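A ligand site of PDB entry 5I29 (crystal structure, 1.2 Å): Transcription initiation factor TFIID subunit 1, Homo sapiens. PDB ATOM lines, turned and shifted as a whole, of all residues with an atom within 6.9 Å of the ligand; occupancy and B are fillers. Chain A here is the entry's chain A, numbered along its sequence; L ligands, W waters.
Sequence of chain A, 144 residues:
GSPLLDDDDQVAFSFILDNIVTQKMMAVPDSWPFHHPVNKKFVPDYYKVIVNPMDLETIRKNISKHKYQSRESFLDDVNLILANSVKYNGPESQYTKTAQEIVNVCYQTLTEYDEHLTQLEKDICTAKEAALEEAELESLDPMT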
ATOM      1  N   TRP A  32     -24.734  19.242  22.751  1.00  0.00           N
ATOM      2  CA  TRP A  32     -25.644  19.259  21.622  1.00  0.00           C
ATOM      3  C   TRP A  32     -24.984  19.548  20.220  1.00  0.00           C
ATOM      4  O   TRP A  32     -25.519  18.981  19.257  1.00  0.00           O
ATOM      5  CB  TRP A  32     -26.720  20.371  21.900  1.00  0.00           C
ATOM      6  CG  TRP A  32     -26.233  21.782  21.922  1.00  0.00           C
ATOM      7  CD1 TRP A  32     -25.869  22.443  23.058  1.00  0.00           C
ATOM      8  CD2 TRP A  32     -25.883  22.649  20.854  1.00  0.00           C
ATOM      9  NE1 TRP A  32     -25.341  23.650  22.789  1.00  0.00           N
ATOM     10  CE2 TRP A  32     -25.319  23.809  21.419  1.00  0.00           C
ATOM     11  CE3 TRP A  32     -25.978  22.581  19.419  1.00  0.00           C
ATOM     12  CZ2 TRP A  32     -24.824  24.842  20.628  1.00  0.00           C
ATOM     13  CZ3 TRP A  32     -25.483  23.646  18.653  1.00  0.00           C
ATOM     14  CH2 TRP A  32     -24.906  24.746  19.288  1.00  0.00           C
ATOM     15  N   PRO A  33     -23.881  20.281  20.045  1.00  0.00           N
ATOM     16  CA  PRO A  33     -23.363  20.396  18.660  1.00  0.00           C
ATOM     17  C   PRO A  33     -23.009  19.073  18.082  1.00  0.00           C
ATOM     18  O   PRO A  33     -22.983  18.991  16.776  1.00  0.00           O
ATOM     19  CB  PRO A  33     -22.098  21.255  18.845  1.00  0.00           C
ATOM     20  CG  PRO A  33     -22.372  22.028  20.152  1.00  0.00           C
ATOM     21  CD  PRO A  33     -23.056  21.035  21.059  1.00  0.00           C
ATOM     22  N   PHE A  34     -22.753  18.055  18.864  1.00  0.00           N
ATOM     23  CA  PHE A  34     -22.251  16.783  18.423  1.00  0.00           C
ATOM     24  C   PHE A  34     -23.323  15.730  18.362  1.00  0.00           C
ATOM     25  O   PHE A  34     -23.032  14.589  17.951  1.00  0.00           O
ATOM     26  CB  PHE A  34     -21.060  16.368  19.330  1.00  0.00           C
ATOM     27  CG  PHE A  34     -20.034  17.435  19.408  1.00  0.00           C
ATOM     28  CD1 PHE A  34     -19.198  17.674  18.296  1.00  0.00           C
ATOM     29  CD2 PHE A  34     -19.897  18.302  20.517  1.00  0.00           C
ATOM     30  CE1 PHE A  34     -18.288  18.722  18.311  1.00  0.00           C
ATOM     31  CE2 PHE A  34     -18.978  19.296  20.553  1.00  0.00           C
ATOM     32  CZ  PHE A  34     -18.148  19.502  19.447  1.00  0.00           C
ATOM     33  N   HIS A  35     -24.537  16.060  18.775  1.00  0.00           N
ATOM     34  CA  HIS A  35     -25.573  15.032  18.837  1.00  0.00           C
ATOM     35  C   HIS A  35     -26.070  14.540  17.476  1.00  0.00           C
ATOM     36  O   HIS A  35     -26.506  13.378  17.346  1.00  0.00           O
ATOM     37  CB  HIS A  35     -26.758  15.566  19.605  1.00  0.00           C
ATOM     38  CG  HIS A  35     -26.504  15.759  21.075  1.00  0.00           C
ATOM     39  ND1 HIS A  35     -27.532  16.234  21.859  1.00  0.00           N
ATOM     40  CD2 HIS A  35     -25.408  15.579  21.815  1.00  0.00           C
ATOM     41  CE1 HIS A  35     -27.018  16.345  23.098  1.00  0.00           C
ATOM     42  NE2 HIS A  35     -25.770  15.894  23.109  1.00  0.00           N
ATOM     43  N   HIS A  36     -26.025  15.406  16.458  1.00  0.00           N
ATOM     44  CA  HIS A  36     -26.622  15.130  15.151  1.00  0.00           C
ATOM     45  C   HIS A  36     -25.682  15.673  14.108  1.00  0.00           C
ATOM     46  O   HIS A  36     -24.813  16.490  14.355  1.00  0.00           O
ATOM     47  CB  HIS A  36     -27.979  15.876  15.034  1.00  0.00           C
ATOM     48  CG  HIS A  36     -28.992  15.428  16.018  1.00  0.00           C
ATOM     49  ND1 HIS A  36     -29.668  14.232  15.896  1.00  0.00           N
ATOM     50  CD2 HIS A  36     -29.411  16.001  17.155  1.00  0.00           C
ATOM     51  CE1 HIS A  36     -30.466  14.056  16.962  1.00  0.00           C
ATOM     52  NE2 HIS A  36     -30.372  15.170  17.708  1.00  0.00           N
ATOM     53  N   PRO A  37     -25.836  15.230  12.812  1.00  0.00           N
ATOM     54  CA  PRO A  37     -24.985  15.803  11.762  1.00  0.00           C
ATOM     55  C   PRO A  37     -25.166  17.326  11.663  1.00  0.00           C
ATOM     56  O   PRO A  37     -26.234  17.859  11.870  1.00  0.00           O
ATOM     57  CB  PRO A  37     -25.523  15.130  10.478  1.00  0.00           C
ATOM     58  CG  PRO A  37     -26.373  14.035  10.928  1.00  0.00           C
ATOM     59  CD  PRO A  37     -26.807  14.239  12.355  1.00  0.00           C
ATOM     60  N   VAL A  38     -24.076  17.992  11.305  1.00  0.00           N
ATOM     61  CA  VAL A  38     -24.207  19.440  11.077  1.00  0.00           C
ATOM     62  C   VAL A  38     -25.075  19.710   9.841  1.00  0.00           C
ATOM     63  O   VAL A  38     -24.956  19.014   8.785  1.00  0.00           O
ATOM     64  CB  VAL A  38     -22.770  19.984  10.830  1.00  0.00           C
ATOM     65  CG1 VAL A  38     -22.872  21.504  10.417  1.00  0.00           C
ATOM     66  CG2 VAL A  38     -21.985  19.897  12.123  1.00  0.00           C
ATOM     67  N   ASN A  39     -25.972  20.610   9.917  1.00  0.00           N
ATOM     68  CA  ASN A  39     -26.779  21.078   8.788  1.00  0.00           C
ATOM     69  C   ASN A  39     -26.127  22.304   8.184  1.00  0.00           C
ATOM     70  O   ASN A  39     -25.965  23.316   8.856  1.00  0.00           O
ATOM     71  CB  ASN A  39     -28.183  21.355   9.344  1.00  0.00           C
ATOM     72  CG  ASN A  39     -29.191  21.599   8.249  1.00  0.00           C
ATOM     73  OD1 ASN A  39     -28.884  22.112   7.151  1.00  0.00           O
ATOM     74  ND2 ASN A  39     -30.430  21.217   8.503  1.00  0.00           N
ATOM     75  N   LYS A  40     -25.805  22.212   6.878  1.00  0.00           N
ATOM     76  CA  LYS A  40     -25.211  23.337   6.213  1.00  0.00           C
ATOM     77  C   LYS A  40     -26.092  24.572   6.228  1.00  0.00           C
ATOM     78  O   LYS A  40     -25.549  25.664   6.082  1.00  0.00           O
ATOM     79  CB  LYS A  40     -24.818  22.954   4.732  1.00  0.00           C
ATOM     80  CG  LYS A  40     -26.015  22.623   3.871  1.00  0.00           C
ATOM     81  CD  LYS A  40     -26.561  23.780   3.048  1.00  0.00           C
ATOM     82  CE  LYS A  40     -27.799  23.245   2.271  1.00  0.00           C
ATOM     83  NZ  LYS A  40     -28.522  24.272   1.455  1.00  0.00           N
ATOM     84  N   LYS A  41     -27.379  24.455   6.426  1.00  0.00           N
ATOM     85  CA  LYS A  41     -28.213  25.648   6.572  1.00  0.00           C
ATOM     86  C   LYS A  41     -27.902  26.422   7.833  1.00  0.00           C
ATOM     87  O   LYS A  41     -28.232  27.591   7.947  1.00  0.00           O
ATOM     88  CB  LYS A  41     -29.661  25.234   6.618  1.00  0.00           C
ATOM     89  CG  LYS A  41     -30.149  24.714   5.261  1.00  0.00           C
ATOM     90  CD  LYS A  41     -31.608  24.399   5.191  1.00  0.00           C
ATOM     91  CE  LYS A  41     -32.010  23.845   3.781  1.00  0.00           C
ATOM     92  NZ  LYS A  41     -33.491  23.669   3.734  1.00  0.00           N
ATOM     93  N   PHE A  42     -27.355  25.756   8.855  1.00  0.00           N
ATOM     94  CA  PHE A  42     -27.018  26.334  10.164  1.00  0.00           C
ATOM     95  C   PHE A  42     -25.537  26.624  10.238  1.00  0.00           C
ATOM     96  O   PHE A  42     -25.173  27.524  11.086  1.00  0.00           O
ATOM     97  CB  PHE A  42     -27.494  25.398  11.263  1.00  0.00           C
ATOM     98  CG  PHE A  42     -28.967  25.015  11.143  1.00  0.00           C
ATOM     99  CD1 PHE A  42     -29.892  25.884  10.535  1.00  0.00           C
ATOM    100  CD2 PHE A  42     -29.416  23.874  11.699  1.00  0.00           C
ATOM    101  CE1 PHE A  42     -31.233  25.512  10.464  1.00  0.00           C
ATOM    102  CE2 PHE A  42     -30.794  23.557  11.640  1.00  0.00           C
ATOM    103  CZ  PHE A  42     -31.659  24.361  10.986  1.00  0.00           C
ATOM    104  N   VAL A  43     -24.663  25.904   9.552  1.00  0.00           N
ATOM    105  CA  VAL A  43     -23.212  26.142   9.622  1.00  0.00           C
ATOM    106  C   VAL A  43     -22.694  26.078   8.158  1.00  0.00           C
ATOM    107  O   VAL A  43     -22.294  25.034   7.661  1.00  0.00           O
ATOM    108  CB  VAL A  43     -22.466  25.112  10.445  1.00  0.00           C
ATOM    109  CG1 VAL A  43     -21.025  25.622  10.639  1.00  0.00           C
ATOM    110  CG2 VAL A  43     -23.102  24.843  11.848  1.00  0.00           C
ATOM    111  N   TYR A  46     -19.273  24.399   6.942  1.00  0.00           N
ATOM    112  CA  TYR A  46     -18.763  23.248   7.678  1.00  0.00           C
ATOM    113  C   TYR A  46     -18.117  22.218   6.773  1.00  0.00           C
ATOM    114  O   TYR A  46     -17.026  21.710   6.984  1.00  0.00           O
ATOM    115  CB  TYR A  46     -19.919  22.596   8.512  1.00  0.00           C
ATOM    116  CG  TYR A  46     -19.346  21.552   9.452  1.00  0.00           C
ATOM    117  CD1 TYR A  46     -18.658  22.015  10.556  1.00  0.00           C
ATOM    118  CD2 TYR A  46     -19.410  20.193   9.235  1.00  0.00           C
ATOM    119  CE1 TYR A  46     -18.091  21.101  11.506  1.00  0.00           C
ATOM    120  CE2 TYR A  46     -18.842  19.260  10.121  1.00  0.00           C
ATOM    121  CZ  TYR A  46     -18.169  19.756  11.232  1.00  0.00           C
ATOM    122  OH  TYR A  46     -17.631  18.813  12.049  1.00  0.00           O
ATOM    123  N   MET A  54     -18.636  13.341  11.146  1.00  0.00           N
ATOM    124  CA  MET A  54     -19.161  12.327  12.035  1.00  0.00           C
ATOM    125  C   MET A  54     -19.867  12.976  13.151  1.00  0.00           C
ATOM    126  O   MET A  54     -19.517  14.080  13.554  1.00  0.00           O
ATOM    127  CB  MET A  54     -18.015  11.393  12.468  1.00  0.00           C
ATOM    128  CG  MET A  54     -18.376  10.180  13.340  1.00  0.00           C
ATOM    129  SD  MET A  54     -19.645   9.139  12.558  1.00  0.00           S
ATOM    130  CE  MET A  54     -18.829   8.717  10.969  1.00  0.00           C
ATOM    131  N   ILE A  81     -15.052  12.638  15.599  1.00  0.00           N
ATOM    132  CA  ILE A  81     -15.778  13.779  16.113  1.00  0.00           C
ATOM    133  C   ILE A  81     -14.856  14.794  16.732  1.00  0.00           C
ATOM    134  O   ILE A  81     -14.957  16.035  16.418  1.00  0.00           O
ATOM    135  CB  ILE A  81     -16.835  13.313  17.170  1.00  0.00           C
ATOM    136  CG1 ILE A  81     -17.853  12.412  16.436  1.00  0.00           C
ATOM    137  CG2 ILE A  81     -17.499  14.521  17.810  1.00  0.00           C
ATOM    138  CD1 ILE A  81     -18.956  11.889  17.417  1.00  0.00           C
ATOM    139  N   ASN A  84     -12.476  16.394  14.026  1.00  0.00           N
ATOM    140  CA  ASN A  84     -13.168  17.391  13.213  1.00  0.00           C
ATOM    141  C   ASN A  84     -13.360  18.687  13.933  1.00  0.00           C
ATOM    142  O   ASN A  84     -13.245  19.758  13.357  1.00  0.00           O
ATOM    143  CB  ASN A  84     -14.531  16.831  12.718  1.00  0.00           C
ATOM    144  CG  ASN A  84     -14.366  15.724  11.654  1.00  0.00           C
ATOM    145  OD1 ASN A  84     -13.327  15.645  11.032  1.00  0.00           O
ATOM    146  ND2 ASN A  84     -15.409  14.993  11.458  1.00  0.00           N
ATOM    147  N   SER A  85     -13.643  18.615  15.261  1.00  0.00           N
ATOM    148  CA  SER A  85     -13.760  19.854  15.995  1.00  0.00           C
ATOM    149  C   SER A  85     -12.400  20.569  16.128  1.00  0.00           C
ATOM    150  O   SER A  85     -12.385  21.795  15.983  1.00  0.00           O
ATOM    151  CB  SER A  85     -14.309  19.615  17.404  1.00  0.00           C
ATOM    152  OG  SER A  85     -14.555  20.854  18.070  1.00  0.00           O
ATOM    153  N   TYR A  88     -12.125  22.238  12.590  1.00  0.00           N
ATOM    154  CA  TYR A  88     -13.058  23.294  12.246  1.00  0.00           C
ATOM    155  C   TYR A  88     -13.051  24.448  13.220  1.00  0.00           C
ATOM    156  O   TYR A  88     -13.160  25.606  12.863  1.00  0.00           O
ATOM    157  CB  TYR A  88     -14.474  22.704  12.119  1.00  0.00           C
ATOM    158  CG  TYR A  88     -15.457  23.693  11.586  1.00  0.00           C
ATOM    159  CD1 TYR A  88     -15.424  24.084  10.261  1.00  0.00           C
ATOM    160  CD2 TYR A  88     -16.355  24.367  12.409  1.00  0.00           C
ATOM    161  CE1 TYR A  88     -16.291  25.204   9.829  1.00  0.00           C
ATOM    162  CE2 TYR A  88     -17.167  25.378  12.037  1.00  0.00           C
ATOM    163  CZ  TYR A  88     -17.088  25.808  10.774  1.00  0.00           C
ATOM    164  OH  TYR A  88     -17.911  26.909  10.386  1.00  0.00           O
ATOM    165  N   ASN A  89     -13.009  24.129  14.538  1.00  0.00           N
ATOM    166  CA  ASN A  89     -13.136  25.120  15.601  1.00  0.00           C
ATOM    167  C   ASN A  89     -11.800  25.527  16.165  1.00  0.00           C
ATOM    168  O   ASN A  89     -11.706  26.618  16.795  1.00  0.00           O
ATOM    169  CB  ASN A  89     -14.034  24.570  16.700  1.00  0.00           C
ATOM    170  CG  ASN A  89     -15.392  24.195  16.173  1.00  0.00           C
ATOM    171  OD1 ASN A  89     -16.060  25.073  15.603  1.00  0.00           O
ATOM    172  ND2 ASN A  89     -15.791  22.957  16.353  1.00  0.00           N
ATOM    173  N   SER A  93     -10.893  25.831  21.189  1.00  0.00           N
ATOM    174  CA  SER A  93     -12.311  26.264  21.191  1.00  0.00           C
ATOM    175  C   SER A  93     -13.093  25.522  22.249  1.00  0.00           C
ATOM    176  O   SER A  93     -12.867  24.312  22.454  1.00  0.00           O
ATOM    177  CB  SER A  93     -12.903  25.980  19.811  1.00  0.00           C
ATOM    178  OG  SER A  93     -14.329  26.117  19.798  1.00  0.00           O
ATOM    179  N   TYR A  95     -15.942  24.355  21.743  1.00  0.00           N
ATOM    180  CA  TYR A  95     -16.499  23.218  21.019  1.00  0.00           C
ATOM    181  C   TYR A  95     -15.602  22.015  21.180  1.00  0.00           C
ATOM    182  O   TYR A  95     -16.065  20.898  21.457  1.00  0.00           O
ATOM    183  CB  TYR A  95     -16.714  23.493  19.527  1.00  0.00           C
ATOM    184  CG  TYR A  95     -17.894  24.380  19.181  1.00  0.00           C
ATOM    185  CD1 TYR A  95     -19.156  23.903  19.228  1.00  0.00           C
ATOM    186  CD2 TYR A  95     -17.671  25.627  18.653  1.00  0.00           C
ATOM    187  CE1 TYR A  95     -20.219  24.735  18.862  1.00  0.00           C
ATOM    188  CE2 TYR A  95     -18.709  26.414  18.247  1.00  0.00           C
ATOM    189  CZ  TYR A  95     -19.971  25.977  18.362  1.00  0.00           C
ATOM    190  OH  TYR A  95     -21.111  26.747  18.024  1.00  0.00           O
HETATM  191  C1  LIG L   1     -26.210  24.396  14.713  1.00  0.00           C
HETATM  192  C2  LIG L   1     -26.652  22.175  13.584  1.00  0.00           C
HETATM  193  C3  LIG L   1     -27.836  21.544  15.644  1.00  0.00           C
HETATM  194  C4  LIG L   1     -25.304  25.233  15.346  1.00  0.00           C
HETATM  195  C5  LIG L   1     -24.436  22.822  14.396  1.00  0.00           C
HETATM  196  C6  LIG L   1     -22.076  23.300  15.116  1.00  0.00           C
HETATM  197  C7  LIG L   1     -24.000  24.898  15.493  1.00  0.00           C
HETATM  198  C8  LIG L   1     -21.706  21.978  15.249  1.00  0.00           C
HETATM  199  C9  LIG L   1     -20.168  20.124  15.389  1.00  0.00           C
HETATM  200  O1  LIG L   1     -18.194  21.955  15.301  1.00  0.00           O
HETATM  201  C10 LIG L   1     -19.338  22.372  15.264  1.00  0.00           C
HETATM  202  N1  LIG L   1     -20.427  21.560  15.324  1.00  0.00           N
HETATM  203  C11 LIG L   1     -19.664  23.781  15.171  1.00  0.00           C
HETATM  204  N2  LIG L   1     -18.828  24.827  15.050  1.00  0.00           N
HETATM  205  C12 LIG L   1     -19.604  25.960  14.876  1.00  0.00           C
HETATM  206  C13 LIG L   1     -20.944  25.651  14.866  1.00  0.00           C
HETATM  207  C14 LIG L   1     -20.996  24.222  15.054  1.00  0.00           C
HETATM  208  C15 LIG L   1     -23.524  23.690  15.033  1.00  0.00           C
HETATM  209  C16 LIG L   1     -25.764  23.143  14.290  1.00  0.00           C
HETATM  210  O2  LIG L   1     -26.429  21.996  12.324  1.00  0.00           O
HETATM  211  N3  LIG L   1     -27.613  21.514  14.184  1.00  0.00           N
HETATM  212  C17 LIG L   1     -28.401  20.548  13.448  1.00  0.00           C
HETATM  213  O   HOH W   1     -16.687  19.835  14.334  1.00  0.00           O
HETATM  214  O   HOH W   2     -28.966  17.455  11.991  1.00  0.00           O
HETATM  215  O   HOH W   3     -25.018  19.405  14.649  1.00  0.00           O
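Merely in contact with the ligand: Pro 33 (3.3 Å), Tyr 95 (3.3 Å), Val 43 (3.4 Å), Tyr 88 (3.5 Å), Phe 42 (3.6 Å), Val 38 (3.6 Å), Trp 32 (3.7 Å), Phe 34 (3.7 Å), Pro 37 (3.8 Å) and Tyr 46 (3.9 Å).
Hydrophobic or aromatic side chains within 4 Å of the ligand: Trp 32, Pro 33, Phe 34, Val 38, Phe 42, Val 43, Tyr 46, Tyr 88 and Tyr 95.
Of the 21 residues printed, 12 come within 4 Å of the ligand.
The nearest printed residue that does not touch the ligand is Ser 85 (4.7 Å).
Water W1 lies within hydrogen-bond range of the side-chain hydroxyl of Tyr 46 (2.7 Å), an oxygen (O1) of the ligand (2.8 Å) and the backbone NH of Ser 85 (3.4 Å).
ND2 of Asn 89 sits at hydrogen-bond distance from OG of Ser 85, 3.0 Å away.
The side-chain amide oxygen of Asn 39 is in hydrogen-bond range of the backbone NH of Lys 41 (2.9 Å).
OG of Ser 93 lies within hydrogen-bond range of N of Tyr 95, 3.1 Å away.
An oxygen (O1) of the ligand lies within hydrogen-bond range of the side-chain amide nitrogen (ND2) of Asn 89 (2.8 Å).
The backbone NH (N) of Asn 39 lies within hydrogen-bond range of an oxygen (O2) of the ligand (2.8 Å).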
